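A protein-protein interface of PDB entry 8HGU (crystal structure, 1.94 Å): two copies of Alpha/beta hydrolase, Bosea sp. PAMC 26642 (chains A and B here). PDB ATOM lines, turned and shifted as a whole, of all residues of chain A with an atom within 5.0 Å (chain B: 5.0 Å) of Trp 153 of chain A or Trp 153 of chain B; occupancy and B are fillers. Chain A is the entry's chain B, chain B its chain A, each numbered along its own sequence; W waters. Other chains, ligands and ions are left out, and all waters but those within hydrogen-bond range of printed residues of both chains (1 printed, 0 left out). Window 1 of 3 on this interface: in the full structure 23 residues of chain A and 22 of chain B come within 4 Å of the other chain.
Of the printed residues of chain B, Asn 150 of chain A touches Ser 156 (2.8 Å). Of the printed residues of chain A, Leu 160 of chain B touches Trp 153. Val 152 of chain A touches none of the printed residues of chain B. Phe 181 of chain A touches none of the printed residues of chain B. The nearest residue of chain A that does not touch Trp 153 of chain B is Leu 162 of chain A (4.2 Å). The nearest printed residue of chain B that does not touch His 180 of chain A is Leu 160 of chain B (4.2 Å).
Val 149 of chain A touches Ser 156 of chain B. Trp 153 of chain A touches Trp 153 of chain B (CB to O, 3.3 Å). CD1 of Phe 157 of chain B touches CZ3 of Trp 153 of chain A, at 3.3 Å. Leu 160 of chain B touches Trp 153 of chain A (CD1 to NE1, 3.7 Å). Ser 156 of chain A touches Trp 153 of chain B. CZ3 of Trp 153 of chain B touches CD1 of Phe 157 of chain A, 3.4 Å away. NE1 of Trp 153 of chain B touches CD1 of Leu 160 of chain A, at 3.7 Å. CD1 of Tyr 177 of chain B touches CD2 of Leu 162 of chain A, at 3.99 Å. CD2 of Leu 162 of chain A touches CB of His 180 of chain B, at 3.9 Å. His 180 of chain A touches Leu 162 of chain B.
Of the 14 printed residues of chain B, 9 touch a printed residue of chain A. Of the 14 printed residues of chain A, 8 touch a printed residue of chain B. Printed residues of chain A that touch a printed residue of chain B: Val 149, Asn 150, Trp 153, Ser 156, Phe 157, Leu 160, Leu 162 and His 180. Hydrophobic or aromatic side chains of chain A that line the printed part of chain B: Trp 153, Phe 157, Leu 160, Leu 162 and His 180. Among the printed residues, 14 pairs touch across the chains.
The side-chain hydroxyl (OG) of Ser 156 of chain A is in hydrogen-bond range of the side-chain amide nitrogen (ND2) of Asn 150 of chain B (2.7 Å). OG of Ser 156 of chain B sits at hydrogen-bond distance from OD1 of Asn 150 of chain A (2.8 Å).
Water W1 lies within hydrogen-bond range of N of Leu 162 of chain A (3.0 Å) and ND1 of His 180 of chain B (3.5 Å).
Asn 150 of chain A touches Ser 156 of chain B, and with the chains exchanged Ser 156 of chain A touches Asn 150 of chain B. Trp 153 of chain A touches its own counterpart, Trp 153 of chain B. Trp 153 of chain A touches Phe 157 of chain B, and with the chains exchanged Phe 157 of chain A touches Trp 153 of chain B. Leu 160 of chain A touches His 180 of chain B, but with the chains exchanged His 180 of chain A does not touch Leu 160 of chain B (4.2 Å). Positions printed for both chains: 149, 150, 151, 152, 153, 154, 155, 156, 157, 160, 162, 177, 180 and 181. Of the 14 pairs that touch across the chains among the printed residues, 11 have their exchanged pair printed and touching as well.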
ATOM      1  N   VAL A 149      30.498   0.775 -37.165  1.00  0.00           N
ATOM      2  CA  VAL A 149      30.097   0.065 -35.927  1.00  0.00           C
ATOM      3  C   VAL A 149      28.997   0.862 -35.197  1.00  0.00           C
ATOM      4  O   VAL A 149      28.131   0.213 -34.568  1.00  0.00           O
ATOM      5  CB  VAL A 149      31.283  -0.263 -35.020  1.00  0.00           C
ATOM      6  CG1 VAL A 149      31.891   0.980 -34.422  1.00  0.00           C
ATOM      7  CG2 VAL A 149      30.856  -1.260 -33.961  1.00  0.00           C
ATOM      8  N   ASN A 150      28.982   2.197 -35.255  1.00  0.00           N
ATOM      9  CA  ASN A 150      27.974   3.003 -34.495  1.00  0.00           C
ATOM     10  C   ASN A 150      26.547   2.803 -35.045  1.00  0.00           C
ATOM     11  O   ASN A 150      25.578   3.131 -34.301  1.00  0.00           O
ATOM     12  CB  ASN A 150      28.307   4.488 -34.443  1.00  0.00           C
ATOM     13  CG  ASN A 150      29.500   4.837 -33.563  1.00  0.00           C
ATOM     14  OD1 ASN A 150      29.906   4.108 -32.653  1.00  0.00           O
ATOM     15  ND2 ASN A 150      30.118   5.955 -33.876  1.00  0.00           N
ATOM     16  N   GLU A 151      26.395   2.345 -36.299  1.00  0.00           N
ATOM     17  CA  GLU A 151      25.078   2.130 -36.955  1.00  0.00           C
ATOM     18  C   GLU A 151      24.484   0.740 -36.647  1.00  0.00           C
ATOM     19  O   GLU A 151      23.243   0.643 -36.673  1.00  0.00           O
ATOM     20  CB  GLU A 151      25.179   2.353 -38.468  1.00  0.00           C
ATOM     21  CG  GLU A 151      25.514   3.777 -38.842  1.00  0.00           C
ATOM     22  CD  GLU A 151      24.379   4.747 -38.527  1.00  0.00           C
ATOM     23  OE1 GLU A 151      23.195   4.299 -38.359  1.00  0.00           O
ATOM     24  OE2 GLU A 151      24.657   5.941 -38.493  1.00  0.00           O
ATOM     25  N   VAL A 152      25.293  -0.284 -36.357  1.00  0.00           N
ATOM     26  CA  VAL A 152      24.832  -1.705 -36.334  1.00  0.00           C
ATOM     27  C   VAL A 152      24.515  -2.161 -34.908  1.00  0.00           C
ATOM     28  O   VAL A 152      24.139  -3.340 -34.750  1.00  0.00           O
ATOM     29  CB  VAL A 152      25.864  -2.625 -37.013  1.00  0.00           C
ATOM     30  CG1 VAL A 152      26.169  -2.122 -38.402  1.00  0.00           C
ATOM     31  CG2 VAL A 152      27.160  -2.762 -36.226  1.00  0.00           C
ATOM     32  N   TRP A 153      24.624  -1.275 -33.905  1.00  0.00           N
ATOM     33  CA  TRP A 153      24.368  -1.655 -32.496  1.00  0.00           C
ATOM     34  C   TRP A 153      23.050  -2.444 -32.401  1.00  0.00           C
ATOM     35  O   TRP A 153      22.982  -3.389 -31.605  1.00  0.00           O
ATOM     36  CB  TRP A 153      24.321  -0.433 -31.581  1.00  0.00           C
ATOM     37  CG  TRP A 153      23.185   0.489 -31.872  1.00  0.00           C
ATOM     38  CD1 TRP A 153      23.207   1.545 -32.723  1.00  0.00           C
ATOM     39  CD2 TRP A 153      21.849   0.424 -31.340  1.00  0.00           C
ATOM     40  NE1 TRP A 153      21.977   2.125 -32.782  1.00  0.00           N
ATOM     41  CE2 TRP A 153      21.129   1.479 -31.931  1.00  0.00           C
ATOM     42  CE3 TRP A 153      21.186  -0.417 -30.429  1.00  0.00           C
ATOM     43  CZ2 TRP A 153      19.783   1.717 -31.641  1.00  0.00           C
ATOM     44  CZ3 TRP A 153      19.872  -0.163 -30.121  1.00  0.00           C
ATOM     45  CH2 TRP A 153      19.179   0.879 -30.737  1.00  0.00           C
ATOM     46  N   TYR A 154      22.022  -2.067 -33.158  1.00  0.00           N
ATOM     47  CA  TYR A 154      20.637  -2.613 -32.984  1.00  0.00           C
ATOM     48  C   TYR A 154      20.651  -4.112 -33.349  1.00  0.00           C
ATOM     49  O   TYR A 154      19.827  -4.888 -32.859  1.00  0.00           O
ATOM     50  CB  TYR A 154      19.632  -1.811 -33.822  1.00  0.00           C
ATOM     51  CG  TYR A 154      19.742  -2.137 -35.290  1.00  0.00           C
ATOM     52  CD1 TYR A 154      20.749  -1.591 -36.057  1.00  0.00           C
ATOM     53  CD2 TYR A 154      18.886  -3.036 -35.911  1.00  0.00           C
ATOM     54  CE1 TYR A 154      20.901  -1.893 -37.396  1.00  0.00           C
ATOM     55  CE2 TYR A 154      19.009  -3.336 -37.260  1.00  0.00           C
ATOM     56  CZ  TYR A 154      20.036  -2.776 -37.994  1.00  0.00           C
ATOM     57  OH  TYR A 154      20.265  -3.066 -39.308  1.00  0.00           O
ATOM     58  N   GLN A 155      21.563  -4.544 -34.220  1.00  0.00           N
ATOM     59  CA  GLN A 155      21.559  -5.937 -34.711  1.00  0.00           C
ATOM     60  C   GLN A 155      21.915  -6.871 -33.540  1.00  0.00           C
ATOM     61  O   GLN A 155      21.376  -7.996 -33.486  1.00  0.00           O
ATOM     62  CB  GLN A 155      22.523  -6.155 -35.863  1.00  0.00           C
ATOM     63  CG  GLN A 155      22.190  -5.286 -37.058  1.00  0.00           C
ATOM     64  CD  GLN A 155      23.216  -5.395 -38.162  1.00  0.00           C
ATOM     65  OE1 GLN A 155      24.239  -6.075 -38.047  1.00  0.00           O
ATOM     66  NE2 GLN A 155      22.932  -4.714 -39.261  1.00  0.00           N
ATOM     67  N   SER A 156      22.760  -6.411 -32.626  1.00  0.00           N
ATOM     68  CA  SER A 156      23.241  -7.179 -31.454  1.00  0.00           C
ATOM     69  C   SER A 156      22.301  -6.960 -30.272  1.00  0.00           C
ATOM     70  O   SER A 156      21.992  -7.922 -29.598  1.00  0.00           O
ATOM     71  CB  SER A 156      24.662  -6.841 -31.168  1.00  0.00           C
ATOM     72  OG  SER A 156      25.504  -7.388 -32.219  1.00  0.00           O
ATOM     73  N   PHE A 157      21.821  -5.750 -30.065  1.00  0.00           N
ATOM     74  CA  PHE A 157      20.886  -5.431 -28.963  1.00  0.00           C
ATOM     75  C   PHE A 157      19.621  -6.279 -29.108  1.00  0.00           C
ATOM     76  O   PHE A 157      19.140  -6.862 -28.101  1.00  0.00           O
ATOM     77  CB  PHE A 157      20.563  -3.951 -28.949  1.00  0.00           C
ATOM     78  CG  PHE A 157      19.442  -3.580 -28.032  1.00  0.00           C
ATOM     79  CD1 PHE A 157      19.586  -3.689 -26.663  1.00  0.00           C
ATOM     80  CD2 PHE A 157      18.252  -3.091 -28.544  1.00  0.00           C
ATOM     81  CE1 PHE A 157      18.550  -3.332 -25.823  1.00  0.00           C
ATOM     82  CE2 PHE A 157      17.236  -2.686 -27.700  1.00  0.00           C
ATOM     83  CZ  PHE A 157      17.386  -2.814 -26.336  1.00  0.00           C
ATOM     84  N   LEU A 160      19.118  -9.893 -27.641  1.00  0.00           N
ATOM     85  CA  LEU A 160      19.030 -10.103 -26.165  1.00  0.00           C
ATOM     86  C   LEU A 160      17.568 -10.100 -25.710  1.00  0.00           C
ATOM     87  O   LEU A 160      16.769  -9.277 -26.223  1.00  0.00           O
ATOM     88  CB  LEU A 160      19.785  -8.960 -25.469  1.00  0.00           C
ATOM     89  CG  LEU A 160      21.222  -8.745 -25.917  1.00  0.00           C
ATOM     90  CD1 LEU A 160      21.739  -7.440 -25.363  1.00  0.00           C
ATOM     91  CD2 LEU A 160      22.107  -9.914 -25.514  1.00  0.00           C
ATOM     92  N   LEU A 162      16.716  -8.709 -23.105  1.00  0.00           N
ATOM     93  CA  LEU A 162      16.589  -7.284 -22.705  1.00  0.00           C
ATOM     94  C   LEU A 162      15.811  -6.463 -23.739  1.00  0.00           C
ATOM     95  O   LEU A 162      14.945  -5.645 -23.339  1.00  0.00           O
ATOM     96  CB  LEU A 162      17.997  -6.696 -22.488  1.00  0.00           C
ATOM     97  CG  LEU A 162      18.045  -5.196 -22.286  1.00  0.00           C
ATOM     98  CD1 LEU A 162      17.288  -4.820 -21.041  1.00  0.00           C
ATOM     99  CD2 LEU A 162      19.492  -4.689 -22.235  1.00  0.00           C
ATOM    100  N   TYR A 177      11.035   3.618 -29.599  1.00  0.00           N
ATOM    101  CA  TYR A 177      12.040   2.742 -30.234  1.00  0.00           C
ATOM    102  C   TYR A 177      11.835   2.734 -31.755  1.00  0.00           C
ATOM    103  O   TYR A 177      12.781   2.966 -32.526  1.00  0.00           O
ATOM    104  CB  TYR A 177      11.927   1.322 -29.680  1.00  0.00           C
ATOM    105  CG  TYR A 177      13.104   0.467 -30.048  1.00  0.00           C
ATOM    106  CD1 TYR A 177      14.346   0.700 -29.478  1.00  0.00           C
ATOM    107  CD2 TYR A 177      13.008  -0.519 -31.020  1.00  0.00           C
ATOM    108  CE1 TYR A 177      15.439  -0.103 -29.796  1.00  0.00           C
ATOM    109  CE2 TYR A 177      14.100  -1.321 -31.349  1.00  0.00           C
ATOM    110  CZ  TYR A 177      15.325  -1.095 -30.743  1.00  0.00           C
ATOM    111  OH  TYR A 177      16.424  -1.842 -31.083  1.00  0.00           O
ATOM    112  N   HIS A 180      12.575   5.983 -33.731  1.00  0.00           N
ATOM    113  CA  HIS A 180      14.034   6.113 -33.949  1.00  0.00           C
ATOM    114  C   HIS A 180      14.392   5.540 -35.323  1.00  0.00           C
ATOM    115  O   HIS A 180      15.080   6.248 -36.043  1.00  0.00           O
ATOM    116  CB  HIS A 180      14.893   5.433 -32.872  1.00  0.00           C
ATOM    117  CG  HIS A 180      16.353   5.448 -33.224  1.00  0.00           C
ATOM    118  ND1 HIS A 180      17.119   6.598 -33.161  1.00  0.00           N
ATOM    119  CD2 HIS A 180      17.166   4.472 -33.693  1.00  0.00           C
ATOM    120  CE1 HIS A 180      18.357   6.316 -33.577  1.00  0.00           C
ATOM    121  NE2 HIS A 180      18.421   5.013 -33.910  1.00  0.00           N
ATOM    122  N   PHE A 181      14.001   4.315 -35.651  1.00  0.00           N
ATOM    123  CA  PHE A 181      14.456   3.625 -36.892  1.00  0.00           C
ATOM    124  C   PHE A 181      13.781   4.254 -38.118  1.00  0.00           C
ATOM    125  O   PHE A 181      14.444   4.454 -39.130  1.00  0.00           O
ATOM    126  CB  PHE A 181      14.273   2.109 -36.781  1.00  0.00           C
ATOM    127  CG  PHE A 181      15.216   1.504 -35.773  1.00  0.00           C
ATOM    128  CD1 PHE A 181      16.533   1.249 -36.109  1.00  0.00           C
ATOM    129  CD2 PHE A 181      14.835   1.332 -34.458  1.00  0.00           C
ATOM    130  CE1 PHE A 181      17.434   0.780 -35.171  1.00  0.00           C
ATOM    131  CE2 PHE A 181      15.733   0.853 -33.516  1.00  0.00           C
ATOM    132  CZ  PHE A 181      17.039   0.591 -33.872  1.00  0.00           C
ATOM    133  N   VAL B 149      31.771  -7.903 -31.862  1.00  0.00           N
ATOM    134  CA  VAL B 149      30.827  -6.826 -32.229  1.00  0.00           C
ATOM    135  C   VAL B 149      29.540  -7.028 -31.432  1.00  0.00           C
ATOM    136  O   VAL B 149      28.875  -6.001 -31.116  1.00  0.00           O
ATOM    137  CB  VAL B 149      30.555  -6.770 -33.753  1.00  0.00           C
ATOM    138  CG1 VAL B 149      29.752  -7.978 -34.214  1.00  0.00           C
ATOM    139  CG2 VAL B 149      29.823  -5.492 -34.117  1.00  0.00           C
ATOM    140  N   ASN B 150      29.235  -8.261 -31.029  1.00  0.00           N
ATOM    141  CA  ASN B 150      27.975  -8.565 -30.315  1.00  0.00           C
ATOM    142  C   ASN B 150      28.073  -8.012 -28.883  1.00  0.00           C
ATOM    143  O   ASN B 150      27.011  -7.723 -28.300  1.00  0.00           O
ATOM    144  CB  ASN B 150      27.638 -10.048 -30.242  1.00  0.00           C
ATOM    145  CG  ASN B 150      27.236 -10.650 -31.577  1.00  0.00           C
ATOM    146  OD1 ASN B 150      27.540 -11.811 -31.914  1.00  0.00           O
ATOM    147  ND2 ASN B 150      26.526  -9.845 -32.325  1.00  0.00           N
ATOM    148  N   GLU B 151      29.272  -7.774 -28.369  1.00  0.00           N
ATOM    149  CA  GLU B 151      29.417  -7.329 -26.953  1.00  0.00           C
ATOM    150  C   GLU B 151      29.405  -5.810 -26.862  1.00  0.00           C
ATOM    151  O   GLU B 151      29.151  -5.354 -25.771  1.00  0.00           O
ATOM    152  CB  GLU B 151      30.711  -7.841 -26.327  1.00  0.00           C
ATOM    153  CG  GLU B 151      30.809  -9.347 -26.224  1.00  0.00           C
ATOM    154  CD  GLU B 151      29.699 -10.022 -25.421  1.00  0.00           C
ATOM    155  OE1 GLU B 151      29.039  -9.350 -24.589  1.00  0.00           O
ATOM    156  OE2 GLU B 151      29.476 -11.208 -25.655  1.00  0.00           O
ATOM    157  N   VAL B 152      29.665  -5.063 -27.951  1.00  0.00           N
ATOM    158  CA  VAL B 152      30.001  -3.606 -27.876  1.00  0.00           C
ATOM    159  C   VAL B 152      28.813  -2.703 -28.231  1.00  0.00           C
ATOM    160  O   VAL B 152      29.006  -1.460 -28.243  1.00  0.00           O
ATOM    161  CB  VAL B 152      31.230  -3.241 -28.715  1.00  0.00           C
ATOM    162  CG1 VAL B 152      32.451  -3.998 -28.225  1.00  0.00           C
ATOM    163  CG2 VAL B 152      31.006  -3.428 -30.224  1.00  0.00           C
ATOM    164  N   TRP B 153      27.659  -3.279 -28.551  1.00  0.00           N
ATOM    165  CA  TRP B 153      26.447  -2.540 -28.998  1.00  0.00           C
ATOM    166  C   TRP B 153      26.151  -1.364 -28.064  1.00  0.00           C
ATOM    167  O   TRP B 153      25.727  -0.291 -28.572  1.00  0.00           O
ATOM    168  CB  TRP B 153      25.251  -3.515 -29.101  1.00  0.00           C
ATOM    169  CG  TRP B 153      24.847  -4.062 -27.766  1.00  0.00           C
ATOM    170  CD1 TRP B 153      25.275  -5.209 -27.173  1.00  0.00           C
ATOM    171  CD2 TRP B 153      23.953  -3.448 -26.818  1.00  0.00           C
ATOM    172  NE1 TRP B 153      24.713  -5.336 -25.943  1.00  0.00           N
ATOM    173  CE2 TRP B 153      23.892  -4.279 -25.700  1.00  0.00           C
ATOM    174  CE3 TRP B 153      23.169  -2.307 -26.827  1.00  0.00           C
ATOM    175  CZ2 TRP B 153      23.100  -4.000 -24.593  1.00  0.00           C
ATOM    176  CZ3 TRP B 153      22.424  -1.994 -25.713  1.00  0.00           C
ATOM    177  CH2 TRP B 153      22.383  -2.833 -24.609  1.00  0.00           C
ATOM    178  N   TYR B 154      26.323  -1.548 -26.749  1.00  0.00           N
ATOM    179  CA  TYR B 154      25.938  -0.558 -25.701  1.00  0.00           C
ATOM    180  C   TYR B 154      26.784   0.719 -25.869  1.00  0.00           C
ATOM    181  O   TYR B 154      26.342   1.784 -25.503  1.00  0.00           O
ATOM    182  CB  TYR B 154      26.067  -1.190 -24.294  1.00  0.00           C
ATOM    183  CG  TYR B 154      27.491  -1.401 -23.852  1.00  0.00           C
ATOM    184  CD1 TYR B 154      28.270  -2.430 -24.365  1.00  0.00           C
ATOM    185  CD2 TYR B 154      28.079  -0.527 -22.955  1.00  0.00           C
ATOM    186  CE1 TYR B 154      29.601  -2.565 -24.011  1.00  0.00           C
ATOM    187  CE2 TYR B 154      29.400  -0.643 -22.583  1.00  0.00           C
ATOM    188  CZ  TYR B 154      30.164  -1.662 -23.121  1.00  0.00           C
ATOM    189  OH  TYR B 154      31.458  -1.790 -22.791  1.00  0.00           O
ATOM    190  N   GLN B 155      28.019   0.608 -26.348  1.00  0.00           N
ATOM    191  CA  GLN B 155      28.950   1.763 -26.411  1.00  0.00           C
ATOM    192  C   GLN B 155      28.409   2.786 -27.422  1.00  0.00           C
ATOM    193  O   GLN B 155      28.579   3.992 -27.205  1.00  0.00           O
ATOM    194  CB  GLN B 155      30.341   1.275 -26.838  1.00  0.00           C
ATOM    195  CG  GLN B 155      31.012   0.350 -25.854  1.00  0.00           C
ATOM    196  CD  GLN B 155      32.358  -0.193 -26.321  1.00  0.00           C
ATOM    197  OE1 GLN B 155      32.845   0.063 -27.432  1.00  0.00           O
ATOM    198  NE2 GLN B 155      32.943  -1.048 -25.507  1.00  0.00           N
ATOM    199  N   SER B 156      27.807   2.305 -28.523  1.00  0.00           N
ATOM    200  CA  SER B 156      27.156   3.147 -29.559  1.00  0.00           C
ATOM    201  C   SER B 156      25.772   3.595 -29.088  1.00  0.00           C
ATOM    202  O   SER B 156      25.440   4.760 -29.214  1.00  0.00           O
ATOM    203  CB  SER B 156      27.086   2.362 -30.839  1.00  0.00           C
ATOM    204  OG  SER B 156      28.394   2.117 -31.326  1.00  0.00           O
ATOM    205  N   PHE B 157      24.971   2.674 -28.585  1.00  0.00           N
ATOM    206  CA  PHE B 157      23.581   2.927 -28.168  1.00  0.00           C
ATOM    207  C   PHE B 157      23.571   4.050 -27.136  1.00  0.00           C
ATOM    208  O   PHE B 157      22.718   4.967 -27.218  1.00  0.00           O
ATOM    209  CB  PHE B 157      22.962   1.659 -27.583  1.00  0.00           C
ATOM    210  CG  PHE B 157      21.593   1.866 -26.979  1.00  0.00           C
ATOM    211  CD1 PHE B 157      20.490   2.106 -27.773  1.00  0.00           C
ATOM    212  CD2 PHE B 157      21.408   1.744 -25.604  1.00  0.00           C
ATOM    213  CE1 PHE B 157      19.230   2.263 -27.203  1.00  0.00           C
ATOM    214  CE2 PHE B 157      20.161   1.921 -25.038  1.00  0.00           C
ATOM    215  CZ  PHE B 157      19.076   2.177 -25.837  1.00  0.00           C
ATOM    216  N   LEU B 160      23.266   7.745 -27.924  1.00  0.00           N
ATOM    217  CA  LEU B 160      22.041   8.298 -28.534  1.00  0.00           C
ATOM    218  C   LEU B 160      21.152   8.923 -27.468  1.00  0.00           C
ATOM    219  O   LEU B 160      21.076   8.338 -26.393  1.00  0.00           O
ATOM    220  CB  LEU B 160      21.314   7.178 -29.263  1.00  0.00           C
ATOM    221  CG  LEU B 160      22.147   6.500 -30.342  1.00  0.00           C
ATOM    222  CD1 LEU B 160      21.427   5.265 -30.845  1.00  0.00           C
ATOM    223  CD2 LEU B 160      22.462   7.458 -31.495  1.00  0.00           C
ATOM    224  N   LEU B 162      18.018   8.435 -27.621  1.00  0.00           N
ATOM    225  CA  LEU B 162      17.121   7.256 -27.418  1.00  0.00           C
ATOM    226  C   LEU B 162      17.457   6.476 -26.130  1.00  0.00           C
ATOM    227  O   LEU B 162      16.531   6.021 -25.482  1.00  0.00           O
ATOM    228  CB  LEU B 162      17.235   6.320 -28.623  1.00  0.00           C
ATOM    229  CG  LEU B 162      16.489   4.995 -28.477  1.00  0.00           C
ATOM    230  CD1 LEU B 162      14.989   5.232 -28.311  1.00  0.00           C
ATOM    231  CD2 LEU B 162      16.775   4.120 -29.669  1.00  0.00           C
ATOM    232  N   TYR B 177      17.713  -2.722 -17.625  1.00  0.00           N
ATOM    233  CA  TYR B 177      18.962  -2.372 -18.346  1.00  0.00           C
ATOM    234  C   TYR B 177      20.195  -2.731 -17.514  1.00  0.00           C
ATOM    235  O   TYR B 177      21.098  -3.402 -18.010  1.00  0.00           O
ATOM    236  CB  TYR B 177      18.935  -0.905 -18.767  1.00  0.00           C
ATOM    237  CG  TYR B 177      19.976  -0.531 -19.783  1.00  0.00           C
ATOM    238  CD1 TYR B 177      19.785  -0.871 -21.122  1.00  0.00           C
ATOM    239  CD2 TYR B 177      21.115   0.177 -19.444  1.00  0.00           C
ATOM    240  CE1 TYR B 177      20.696  -0.521 -22.090  1.00  0.00           C
ATOM    241  CE2 TYR B 177      22.053   0.523 -20.406  1.00  0.00           C
ATOM    242  CZ  TYR B 177      21.834   0.171 -21.730  1.00  0.00           C
ATOM    243  OH  TYR B 177      22.730   0.452 -22.695  1.00  0.00           O
ATOM    244  N   HIS B 180      21.012  -6.493 -16.835  1.00  0.00           N
ATOM    245  CA  HIS B 180      21.672  -7.153 -17.992  1.00  0.00           C
ATOM    246  C   HIS B 180      23.216  -7.091 -17.847  1.00  0.00           C
ATOM    247  O   HIS B 180      23.866  -8.131 -18.011  1.00  0.00           O
ATOM    248  CB  HIS B 180      21.222  -6.543 -19.336  1.00  0.00           C
ATOM    249  CG  HIS B 180      22.105  -7.028 -20.422  1.00  0.00           C
ATOM    250  ND1 HIS B 180      21.963  -8.269 -20.919  1.00  0.00           N
ATOM    251  CD2 HIS B 180      23.187  -6.480 -21.037  1.00  0.00           C
ATOM    252  CE1 HIS B 180      22.914  -8.511 -21.812  1.00  0.00           C
ATOM    253  NE2 HIS B 180      23.670  -7.419 -21.926  1.00  0.00           N
ATOM    254  N   PHE B 181      23.795  -5.921 -17.568  1.00  0.00           N
ATOM    255  CA  PHE B 181      25.268  -5.757 -17.486  1.00  0.00           C
ATOM    256  C   PHE B 181      25.811  -6.473 -16.250  1.00  0.00           C
ATOM    257  O   PHE B 181      26.874  -7.196 -16.299  1.00  0.00           O
ATOM    258  CB  PHE B 181      25.640  -4.280 -17.538  1.00  0.00           C
ATOM    259  CG  PHE B 181      25.275  -3.680 -18.865  1.00  0.00           C
ATOM    260  CD1 PHE B 181      26.082  -3.850 -19.975  1.00  0.00           C
ATOM    261  CD2 PHE B 181      24.085  -2.984 -19.003  1.00  0.00           C
ATOM    262  CE1 PHE B 181      25.706  -3.328 -21.206  1.00  0.00           C
ATOM    263  CE2 PHE B 181      23.715  -2.463 -20.228  1.00  0.00           C
ATOM    264  CZ  PHE B 181      24.540  -2.612 -21.320  1.00  0.00           C
HETATM  265  O   HOH W   1      19.192 -10.053 -22.030  1.00  0.00           O
